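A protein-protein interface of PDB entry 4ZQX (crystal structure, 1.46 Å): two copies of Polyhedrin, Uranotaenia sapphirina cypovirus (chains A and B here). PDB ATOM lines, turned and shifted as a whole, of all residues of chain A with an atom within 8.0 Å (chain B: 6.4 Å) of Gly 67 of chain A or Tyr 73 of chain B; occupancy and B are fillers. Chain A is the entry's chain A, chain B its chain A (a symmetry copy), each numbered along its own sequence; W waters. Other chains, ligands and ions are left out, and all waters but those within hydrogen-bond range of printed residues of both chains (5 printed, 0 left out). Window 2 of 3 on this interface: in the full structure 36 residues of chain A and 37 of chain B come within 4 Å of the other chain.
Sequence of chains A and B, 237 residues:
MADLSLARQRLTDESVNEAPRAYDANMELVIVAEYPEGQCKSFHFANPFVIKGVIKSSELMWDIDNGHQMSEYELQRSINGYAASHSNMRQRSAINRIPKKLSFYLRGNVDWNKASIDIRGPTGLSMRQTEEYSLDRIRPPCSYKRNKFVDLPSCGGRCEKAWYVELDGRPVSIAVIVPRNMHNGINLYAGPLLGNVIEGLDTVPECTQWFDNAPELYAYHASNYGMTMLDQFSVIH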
ATOM      1  N   CYS A  40      12.670   2.070  -7.948  1.00  0.00           N
ATOM      2  CA  CYS A  40      12.763   0.815  -8.687  1.00  0.00           C
ATOM      3  C   CYS A  40      12.145  -0.313  -7.898  1.00  0.00           C
ATOM      4  O   CYS A  40      12.234  -0.355  -6.657  1.00  0.00           O
ATOM      5  CB  CYS A  40      14.223   0.432  -8.954  1.00  0.00           C
ATOM      6  SG  CYS A  40      15.155   1.577  -9.984  1.00  0.00           S
ATOM      7  N   LYS A  41      11.531  -1.229  -8.633  1.00  0.00           N
ATOM      8  CA  LYS A  41      11.048  -2.483  -8.078  1.00  0.00           C
ATOM      9  C   LYS A  41      11.714  -3.595  -8.870  1.00  0.00           C
ATOM     10  O   LYS A  41      11.728  -3.554 -10.093  1.00  0.00           O
ATOM     11  CB  LYS A  41       9.531  -2.554  -8.229  1.00  0.00           C
ATOM     12  CG  LYS A  41       8.822  -3.212  -7.112  1.00  0.00           C
ATOM     13  CD  LYS A  41       7.318  -2.922  -7.142  1.00  0.00           C
ATOM     14  CE  LYS A  41       6.585  -4.073  -6.516  1.00  0.00           C
ATOM     15  NZ  LYS A  41       5.134  -3.849  -6.413  1.00  0.00           N
ATOM     16  N   TRP A  62       3.915   0.940  -8.763  1.00  0.00           N
ATOM     17  CA  TRP A  62       4.613   1.370  -7.567  1.00  0.00           C
ATOM     18  C   TRP A  62       3.566   1.478  -6.477  1.00  0.00           C
ATOM     19  O   TRP A  62       2.620   2.265  -6.584  1.00  0.00           O
ATOM     20  CB  TRP A  62       5.331   2.703  -7.770  1.00  0.00           C
ATOM     21  CG  TRP A  62       6.009   3.150  -6.536  1.00  0.00           C
ATOM     22  CD1 TRP A  62       5.625   4.155  -5.707  1.00  0.00           C
ATOM     23  CD2 TRP A  62       7.190   2.578  -5.961  1.00  0.00           C
ATOM     24  NE1 TRP A  62       6.500   4.255  -4.647  1.00  0.00           N
ATOM     25  CE2 TRP A  62       7.474   3.302  -4.786  1.00  0.00           C
ATOM     26  CE3 TRP A  62       8.044   1.532  -6.335  1.00  0.00           C
ATOM     27  CZ2 TRP A  62       8.569   3.005  -3.971  1.00  0.00           C
ATOM     28  CZ3 TRP A  62       9.136   1.248  -5.534  1.00  0.00           C
ATOM     29  CH2 TRP A  62       9.390   1.981  -4.369  1.00  0.00           C
ATOM     30  N   ASP A  63       3.732   0.678  -5.431  1.00  0.00           N
ATOM     31  CA  ASP A  63       2.649   0.421  -4.476  1.00  0.00           C
ATOM     32  C   ASP A  63       2.878   0.940  -3.055  1.00  0.00           C
ATOM     33  O   ASP A  63       2.240   0.480  -2.100  1.00  0.00           O
ATOM     34  CB  ASP A  63       2.323  -1.078  -4.482  1.00  0.00           C
ATOM     35  CG  ASP A  63       3.539  -1.957  -4.281  1.00  0.00           C
ATOM     36  OD1 ASP A  63       4.682  -1.495  -4.432  1.00  0.00           O
ATOM     37  OD2 ASP A  63       3.333  -3.141  -3.976  1.00  0.00           O
ATOM     38  N   ILE A  64       3.741   1.938  -2.931  1.00  0.00           N
ATOM     39  CA  ILE A  64       4.053   2.526  -1.631  1.00  0.00           C
ATOM     40  C   ILE A  64       3.438   3.910  -1.548  1.00  0.00           C
ATOM     41  O   ILE A  64       3.621   4.739  -2.450  1.00  0.00           O
ATOM     42  CB  ILE A  64       5.576   2.597  -1.419  1.00  0.00           C
ATOM     43  CG1 ILE A  64       6.213   1.241  -1.741  1.00  0.00           C
ATOM     44  CG2 ILE A  64       5.921   3.034   0.008  1.00  0.00           C
ATOM     45  CD1 ILE A  64       5.588   0.038  -1.017  1.00  0.00           C
ATOM     46  N   ASP A  65       2.718   4.159  -0.456  1.00  0.00           N
ATOM     47  CA  ASP A  65       2.028   5.424  -0.241  1.00  0.00           C
ATOM     48  C   ASP A  65       2.305   5.863   1.183  1.00  0.00           C
ATOM     49  O   ASP A  65       1.840   5.237   2.137  1.00  0.00           O
ATOM     50  CB  ASP A  65       0.521   5.263  -0.479  1.00  0.00           C
ATOM     51  CG  ASP A  65      -0.239   6.577  -0.390  1.00  0.00           C
ATOM     52  OD1 ASP A  65       0.347   7.650  -0.663  1.00  0.00           O
ATOM     53  OD2 ASP A  65      -1.440   6.520  -0.050  1.00  0.00           O
ATOM     54  N   ASN A  66       3.082   6.938   1.303  1.00  0.00           N
ATOM     55  CA  ASN A  66       3.482   7.475   2.597  1.00  0.00           C
ATOM     56  C   ASN A  66       4.006   6.381   3.536  1.00  0.00           C
ATOM     57  O   ASN A  66       3.606   6.300   4.704  1.00  0.00           O
ATOM     58  CB  ASN A  66       2.316   8.246   3.232  1.00  0.00           C
ATOM     59  CG  ASN A  66       1.936   9.497   2.438  1.00  0.00           C
ATOM     60  OD1 ASN A  66       2.799  10.292   2.059  1.00  0.00           O
ATOM     61  ND2 ASN A  66       0.641   9.667   2.173  1.00  0.00           N
ATOM     62  N   GLY A  67       4.883   5.531   3.012  1.00  0.00           N
ATOM     63  CA  GLY A  67       5.558   4.535   3.817  1.00  0.00           C
ATOM     64  C   GLY A  67       4.832   3.225   4.038  1.00  0.00           C
ATOM     65  O   GLY A  67       5.375   2.332   4.697  1.00  0.00           O
ATOM     66  N   HIS A  68       3.616   3.101   3.513  1.00  0.00           N
ATOM     67  CA  HIS A  68       2.845   1.870   3.668  1.00  0.00           C
ATOM     68  C   HIS A  68       2.541   1.261   2.307  1.00  0.00           C
ATOM     69  O   HIS A  68       2.436   1.967   1.309  1.00  0.00           O
ATOM     70  CB  HIS A  68       1.555   2.111   4.476  1.00  0.00           C
ATOM     71  CG  HIS A  68       0.421   2.684   3.682  1.00  0.00           C
ATOM     72  ND1 HIS A  68       0.003   3.991   3.819  1.00  0.00           N
ATOM     73  CD2 HIS A  68      -0.408   2.119   2.771  1.00  0.00           C
ATOM     74  CE1 HIS A  68      -1.020   4.211   3.013  1.00  0.00           C
ATOM     75  NE2 HIS A  68      -1.288   3.092   2.364  1.00  0.00           N
ATOM     76  N   GLN A  69       2.422  -0.058   2.273  1.00  0.00           N
ATOM     77  CA  GLN A  69       2.137  -0.756   1.028  1.00  0.00           C
ATOM     78  C   GLN A  69       0.644  -0.774   0.763  1.00  0.00           C
ATOM     79  O   GLN A  69      -0.145  -1.130   1.638  1.00  0.00           O
ATOM     80  CB  GLN A  69       2.673  -2.183   1.064  1.00  0.00           C
ATOM     81  CG  GLN A  69       2.584  -2.858  -0.284  1.00  0.00           C
ATOM     82  CD  GLN A  69       3.205  -4.231  -0.289  1.00  0.00           C
ATOM     83  OE1 GLN A  69       3.694  -4.714   0.735  1.00  0.00           O
ATOM     84  NE2 GLN A  69       3.196  -4.875  -1.455  1.00  0.00           N
ATOM     85  N   MET A  70       0.274  -0.396  -0.460  1.00  0.00           N
ATOM     86  CA  MET A  70      -1.120  -0.366  -0.888  1.00  0.00           C
ATOM     87  C   MET A  70      -1.629  -1.778  -1.161  1.00  0.00           C
ATOM     88  O   MET A  70      -0.861  -2.680  -1.488  1.00  0.00           O
ATOM     89  CB  MET A  70      -1.248   0.496  -2.142  1.00  0.00           C
ATOM     90  CG  MET A  70      -0.782   1.904  -1.925  1.00  0.00           C
ATOM     91  SD  MET A  70      -0.583   2.787  -3.473  1.00  0.00           S
ATOM     92  CE  MET A  70      -2.267   2.995  -4.009  1.00  0.00           C
ATOM     93  N   THR A 208      10.865 -10.220  -4.433  1.00  0.00           N
ATOM     94  CA  THR A 208      10.529  -8.872  -4.865  1.00  0.00           C
ATOM     95  C   THR A 208      11.215  -7.900  -3.923  1.00  0.00           C
ATOM     96  O   THR A 208      11.148  -8.071  -2.698  1.00  0.00           O
ATOM     97  CB  THR A 208       9.006  -8.618  -4.792  1.00  0.00           C
ATOM     98  OG1 THR A 208       8.319  -9.549  -5.634  1.00  0.00           O
ATOM     99  CG2 THR A 208       8.646  -7.186  -5.217  1.00  0.00           C
ATOM    100  N   GLN A 209      11.856  -6.877  -4.485  1.00  0.00           N
ATOM    101  CA  GLN A 209      12.494  -5.836  -3.674  1.00  0.00           C
ATOM    102  C   GLN A 209      12.127  -4.458  -4.181  1.00  0.00           C
ATOM    103  O   GLN A 209      11.867  -4.265  -5.371  1.00  0.00           O
ATOM    104  CB  GLN A 209      14.015  -6.008  -3.668  1.00  0.00           C
ATOM    105  CG  GLN A 209      14.492  -7.225  -2.888  1.00  0.00           C
ATOM    106  CD  GLN A 209      15.984  -7.489  -3.074  1.00  0.00           C
ATOM    107  OE1 GLN A 209      16.448  -7.728  -4.184  1.00  0.00           O
ATOM    108  NE2 GLN A 209      16.740  -7.425  -1.991  1.00  0.00           N
ATOM    109  N   TRP A 210      12.113  -3.509  -3.250  1.00  0.00           N
ATOM    110  CA  TRP A 210      11.786  -2.113  -3.511  1.00  0.00           C
ATOM    111  C   TRP A 210      13.013  -1.266  -3.223  1.00  0.00           C
ATOM    112  O   TRP A 210      13.668  -1.469  -2.208  1.00  0.00           O
ATOM    113  CB  TRP A 210      10.686  -1.644  -2.565  1.00  0.00           C
ATOM    114  CG  TRP A 210       9.337  -2.239  -2.796  1.00  0.00           C
ATOM    115  CD1 TRP A 210       8.281  -1.639  -3.410  1.00  0.00           C
ATOM    116  CD2 TRP A 210       8.888  -3.537  -2.395  1.00  0.00           C
ATOM    117  NE1 TRP A 210       7.198  -2.483  -3.424  1.00  0.00           N
ATOM    118  CE2 TRP A 210       7.545  -3.657  -2.806  1.00  0.00           C
ATOM    119  CE3 TRP A 210       9.488  -4.608  -1.735  1.00  0.00           C
ATOM    120  CZ2 TRP A 210       6.792  -4.804  -2.584  1.00  0.00           C
ATOM    121  CZ3 TRP A 210       8.732  -5.761  -1.512  1.00  0.00           C
ATOM    122  CH2 TRP A 210       7.393  -5.843  -1.933  1.00  0.00           C
ATOM    123  N   PHE A 211      13.316  -0.315  -4.100  1.00  0.00           N
ATOM    124  CA  PHE A 211      14.432   0.611  -3.898  1.00  0.00           C
ATOM    125  C   PHE A 211      13.986   2.039  -4.215  1.00  0.00           C
ATOM    126  O   PHE A 211      13.178   2.260  -5.123  1.00  0.00           O
ATOM    127  CB  PHE A 211      15.613   0.234  -4.796  1.00  0.00           C
ATOM    128  CG  PHE A 211      16.098  -1.174  -4.604  1.00  0.00           C
ATOM    129  CD1 PHE A 211      17.045  -1.476  -3.635  1.00  0.00           C
ATOM    130  CD2 PHE A 211      15.611  -2.191  -5.389  1.00  0.00           C
ATOM    131  CE1 PHE A 211      17.496  -2.789  -3.460  1.00  0.00           C
ATOM    132  CE2 PHE A 211      16.051  -3.502  -5.209  1.00  0.00           C
ATOM    133  CZ  PHE A 211      16.991  -3.792  -4.244  1.00  0.00           C
ATOM    134  N   ASP A 212      14.514   3.012  -3.481  1.00  0.00           N
ATOM    135  CA  ASP A 212      14.106   4.401  -3.703  1.00  0.00           C
ATOM    136  C   ASP A 212      14.803   5.043  -4.886  1.00  0.00           C
ATOM    137  O   ASP A 212      14.313   6.026  -5.437  1.00  0.00           O
ATOM    138  CB  ASP A 212      14.305   5.253  -2.443  1.00  0.00           C
ATOM    139  CG  ASP A 212      13.249   4.981  -1.412  1.00  0.00           C
ATOM    140  OD1 ASP A 212      12.088   5.258  -1.703  1.00  0.00           O
ATOM    141  OD2 ASP A 212      13.560   4.474  -0.327  1.00  0.00           O
ATOM    142  N   MET B  70       1.672  -7.561   8.956  1.00  0.00           N
ATOM    143  CA  MET B  70       2.648  -6.691   8.311  1.00  0.00           C
ATOM    144  C   MET B  70       2.699  -6.959   6.810  1.00  0.00           C
ATOM    145  O   MET B  70       2.391  -8.056   6.348  1.00  0.00           O
ATOM    146  CB  MET B  70       4.022  -6.915   8.937  1.00  0.00           C
ATOM    147  CG  MET B  70       4.037  -6.644  10.411  1.00  0.00           C
ATOM    148  SD  MET B  70       5.528  -7.265  11.190  1.00  0.00           S
ATOM    149  CE  MET B  70       6.772  -6.159  10.561  1.00  0.00           C
ATOM    150  N   SER B  71       3.089  -5.950   6.044  1.00  0.00           N
ATOM    151  CA  SER B  71       3.161  -6.079   4.591  1.00  0.00           C
ATOM    152  C   SER B  71       4.477  -6.723   4.124  1.00  0.00           C
ATOM    153  O   SER B  71       5.478  -6.729   4.854  1.00  0.00           O
ATOM    154  CB  SER B  71       3.032  -4.698   3.964  1.00  0.00           C
ATOM    155  OG  SER B  71       4.201  -3.956   4.230  1.00  0.00           O
ATOM    156  N   GLU B  72       4.475  -7.257   2.899  1.00  0.00           N
ATOM    157  CA  GLU B  72       5.698  -7.806   2.315  1.00  0.00           C
ATOM    158  C   GLU B  72       6.780  -6.735   2.230  1.00  0.00           C
ATOM    159  O   GLU B  72       7.945  -7.023   2.420  1.00  0.00           O
ATOM    160  CB  GLU B  72       5.443  -8.416   0.934  1.00  0.00           C
ATOM    161  CG  GLU B  72       6.692  -9.055   0.336  1.00  0.00           C
ATOM    162  CD  GLU B  72       6.460  -9.754  -0.985  1.00  0.00           C
ATOM    163  OE1 GLU B  72       5.405  -9.540  -1.624  1.00  0.00           O
ATOM    164  OE2 GLU B  72       7.360 -10.518  -1.387  1.00  0.00           O
ATOM    165  N   TYR B  73       6.385  -5.505   1.946  1.00  0.00           N
ATOM    166  CA  TYR B  73       7.325  -4.387   1.859  1.00  0.00           C
ATOM    167  C   TYR B  73       8.118  -4.213   3.159  1.00  0.00           C
ATOM    168  O   TYR B  73       9.354  -4.128   3.154  1.00  0.00           O
ATOM    169  CB  TYR B  73       6.546  -3.099   1.542  1.00  0.00           C
ATOM    170  CG  TYR B  73       7.346  -1.825   1.585  1.00  0.00           C
ATOM    171  CD1 TYR B  73       8.253  -1.520   0.588  1.00  0.00           C
ATOM    172  CD2 TYR B  73       7.164  -0.912   2.605  1.00  0.00           C
ATOM    173  CE1 TYR B  73       8.966  -0.348   0.609  1.00  0.00           C
ATOM    174  CE2 TYR B  73       7.869   0.256   2.641  1.00  0.00           C
ATOM    175  CZ  TYR B  73       8.773   0.533   1.640  1.00  0.00           C
ATOM    176  OH  TYR B  73       9.489   1.702   1.668  1.00  0.00           O
ATOM    177  N   GLU B  74       7.405  -4.161   4.275  1.00  0.00           N
ATOM    178  CA  GLU B  74       8.047  -3.994   5.578  1.00  0.00           C
ATOM    179  C   GLU B  74       8.924  -5.180   5.940  1.00  0.00           C
ATOM    180  O   GLU B  74      10.026  -5.010   6.479  1.00  0.00           O
ATOM    181  CB  GLU B  74       6.998  -3.885   6.675  1.00  0.00           C
ATOM    182  CG  GLU B  74       6.077  -2.734   6.618  1.00  0.00           C
ATOM    183  CD  GLU B  74       5.013  -2.913   7.681  1.00  0.00           C
ATOM    184  OE1 GLU B  74       5.324  -2.633   8.851  1.00  0.00           O
ATOM    185  OE2 GLU B  74       3.901  -3.397   7.363  1.00  0.00           O
ATOM    186  N   LEU B  75       8.417  -6.386   5.691  1.00  0.00           N
ATOM    187  CA  LEU B  75       9.183  -7.590   6.017  1.00  0.00           C
ATOM    188  C   LEU B  75      10.452  -7.695   5.159  1.00  0.00           C
ATOM    189  O   LEU B  75      11.532  -8.012   5.662  1.00  0.00           O
ATOM    190  CB  LEU B  75       8.312  -8.832   5.836  1.00  0.00           C
ATOM    191  CG  LEU B  75       7.132  -8.880   6.815  1.00  0.00           C
ATOM    192  CD1 LEU B  75       6.089  -9.905   6.389  1.00  0.00           C
ATOM    193  CD2 LEU B  75       7.617  -9.182   8.231  1.00  0.00           C
ATOM    194  N   GLN B  76      10.323  -7.440   3.862  1.00  0.00           N
ATOM    195  CA  GLN B  76      11.477  -7.548   2.984  1.00  0.00           C
ATOM    196  C   GLN B  76      12.519  -6.510   3.373  1.00  0.00           C
ATOM    197  O   GLN B  76      13.722  -6.769   3.278  1.00  0.00           O
ATOM    198  CB  GLN B  76      11.091  -7.380   1.522  1.00  0.00           C
ATOM    199  CG  GLN B  76      12.244  -7.656   0.542  1.00  0.00           C
ATOM    200  CD  GLN B  76      12.760  -9.081   0.630  1.00  0.00           C
ATOM    201  OE1 GLN B  76      11.984 -10.037   0.677  1.00  0.00           O
ATOM    202  NE2 GLN B  76      14.076  -9.231   0.656  1.00  0.00           N
ATOM    203  N   ARG B  77      12.069  -5.348   3.841  1.00  0.00           N
ATOM    204  CA  ARG B  77      13.013  -4.310   4.268  1.00  0.00           C
ATOM    205  C   ARG B  77      13.929  -4.840   5.372  1.00  0.00           C
ATOM    206  O   ARG B  77      15.136  -4.616   5.338  1.00  0.00           O
ATOM    207  CB  ARG B  77      12.265  -3.057   4.741  1.00  0.00           C
ATOM    208  CG  ARG B  77      13.178  -1.879   5.105  1.00  0.00           C
ATOM    209  CD  ARG B  77      12.361  -0.621   5.329  1.00  0.00           C
ATOM    210  NE  ARG B  77      11.303  -0.843   6.319  1.00  0.00           N
ATOM    211  CZ  ARG B  77      10.190  -0.117   6.422  1.00  0.00           C
ATOM    212  NH1 ARG B  77       9.968   0.899   5.593  1.00  0.00           N
ATOM    213  NH2 ARG B  77       9.290  -0.411   7.357  1.00  0.00           N
ATOM    214  N   SER B  78      13.362  -5.579   6.325  1.00  0.00           N
ATOM    215  CA  SER B  78      14.143  -6.126   7.434  1.00  0.00           C
ATOM    216  C   SER B  78      15.082  -7.235   6.975  1.00  0.00           C
ATOM    217  O   SER B  78      16.237  -7.303   7.394  1.00  0.00           O
ATOM    218  CB  SER B  78      13.223  -6.641   8.553  1.00  0.00           C
ATOM    219  OG  SER B  78      12.509  -5.569   9.152  1.00  0.00           O
HETATM  220  O   HOH W   1      10.028 -10.713  -1.662  1.00  0.00           O
HETATM  221  O   HOH W   2       1.851  -7.542   1.500  1.00  0.00           O
HETATM  222  O   HOH W   3       3.852  -7.513  -2.211  1.00  0.00           O
HETATM  223  O   HOH W   4       5.647 -10.019  -4.252  1.00  0.00           O
HETATM  224  O   HOH W   5       3.292  -1.297   4.835  1.00  0.00           O
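OE1 of Gln 69 of chain A sits at hydrogen-bond distance from N of Glu 72 of chain B (3.4 Å). The side-chain amide oxygen (OE1) of Gln 69 of chain A is in hydrogen-bond range of the backbone NH (N) of Tyr 73 of chain B, at 3.1 Å.
Of the 9 printed residues of chain B, 4 touch a printed residue of chain A. Of the 16 printed residues of chain A, 5 touch a printed residue of chain B. Hydrophobic or aromatic side chains of chain A that line the printed part of chain B: Ile 64 and Trp 210. Among the printed residues, no Asp or Glu carboxylate lies within 4 Å of a Lys or Arg side-chain nitrogen of the other chain.
Among the printed residues, merely in contact across the chains: Gln 69 of chain A with Ser 71 of chain B, Thr 208 of chain A with Gln 76 of chain B, Ile 64 of chain A with Tyr 73 of chain B, Trp 210 of chain A with Tyr 73 of chain B, Gly 67 of chain A with Tyr 73 of chain B and Trp 210 of chain A with Glu 72 of chain B.
Of chain B, only Tyr 73 comes within 4 Å of Gly 67 of chain A. Of the printed residues of chain B, Gln 69 of chain A touches Ser 71 (3.3 Å), Glu 72 (3.4 Å) and Tyr 73 (3.1 Å). Of the printed residues of chain B, Trp 210 of chain A touches Glu 72 (3.99 Å) and Tyr 73 (3.6 Å). Of the printed residues of chain B, Ile 64 of chain A touches Tyr 73. Printed residues of chain B within 4 Å of Thr 208 of chain A: Gln 76. His 68 of chain A touches none of the printed residues of chain B. Asp 212 of chain A touches none of the printed residues of chain B. The nearest residue of chain B that does not touch Gly 67 of chain A is Arg 77 of chain B (4.9 Å). The nearest printed residue of chain A that does not touch Tyr 73 of chain B is His 68 of chain A (5.1 Å). The nearest printed residue of chain B that does not touch Ile 64 of chain A is Ser 71 of chain B (6.7 Å).
Water W3 bridges the side-chain carboxylate of Glu 72 of chain B and the side-chain amide nitrogen of Gln 69 of chain A. Water W4 lies within hydrogen-bond range of the side-chain carboxylate (OE1) of Glu 72 of chain B (2.7 Å) and the side-chain hydroxyl (OG1) of Thr 208 of chain A (3.0 Å). Water W1 lies within hydrogen-bond range of OE2 of Glu 72 of chain B, N of Thr 208 of chain A and OE1 of Gln 76 of chain B. Water W5 lies within hydrogen-bond range of OG of Ser 71 of chain B (2.9 Å), N of Gln 69 of chain A (3.0 Å) and OE2 of Glu 74 of chain B (3.3 Å). Water W2 bridges N of Glu 72 of chain B (3.0 Å) and OE1 of Gln 69 of chain A (3.5 Å).
NE2 of Gln 69 of chain A lies within hydrogen-bond range of OD2 of Asp 63 of chain A (3.1 Å). The indole nitrogen of Trp 210 of chain A lies within hydrogen-bond range of the side-chain carboxylate of Asp 63 of chain A, at 2.9 Å. N of Ser 71 of chain B lies within hydrogen-bond range of OE2 of Glu 74 of chain B, at 3.0 Å.
Position printed for both chains: 70. Of the 8 pairs that touch across the chains among the printed residues, none has its exchanged pair printed and touching as well.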
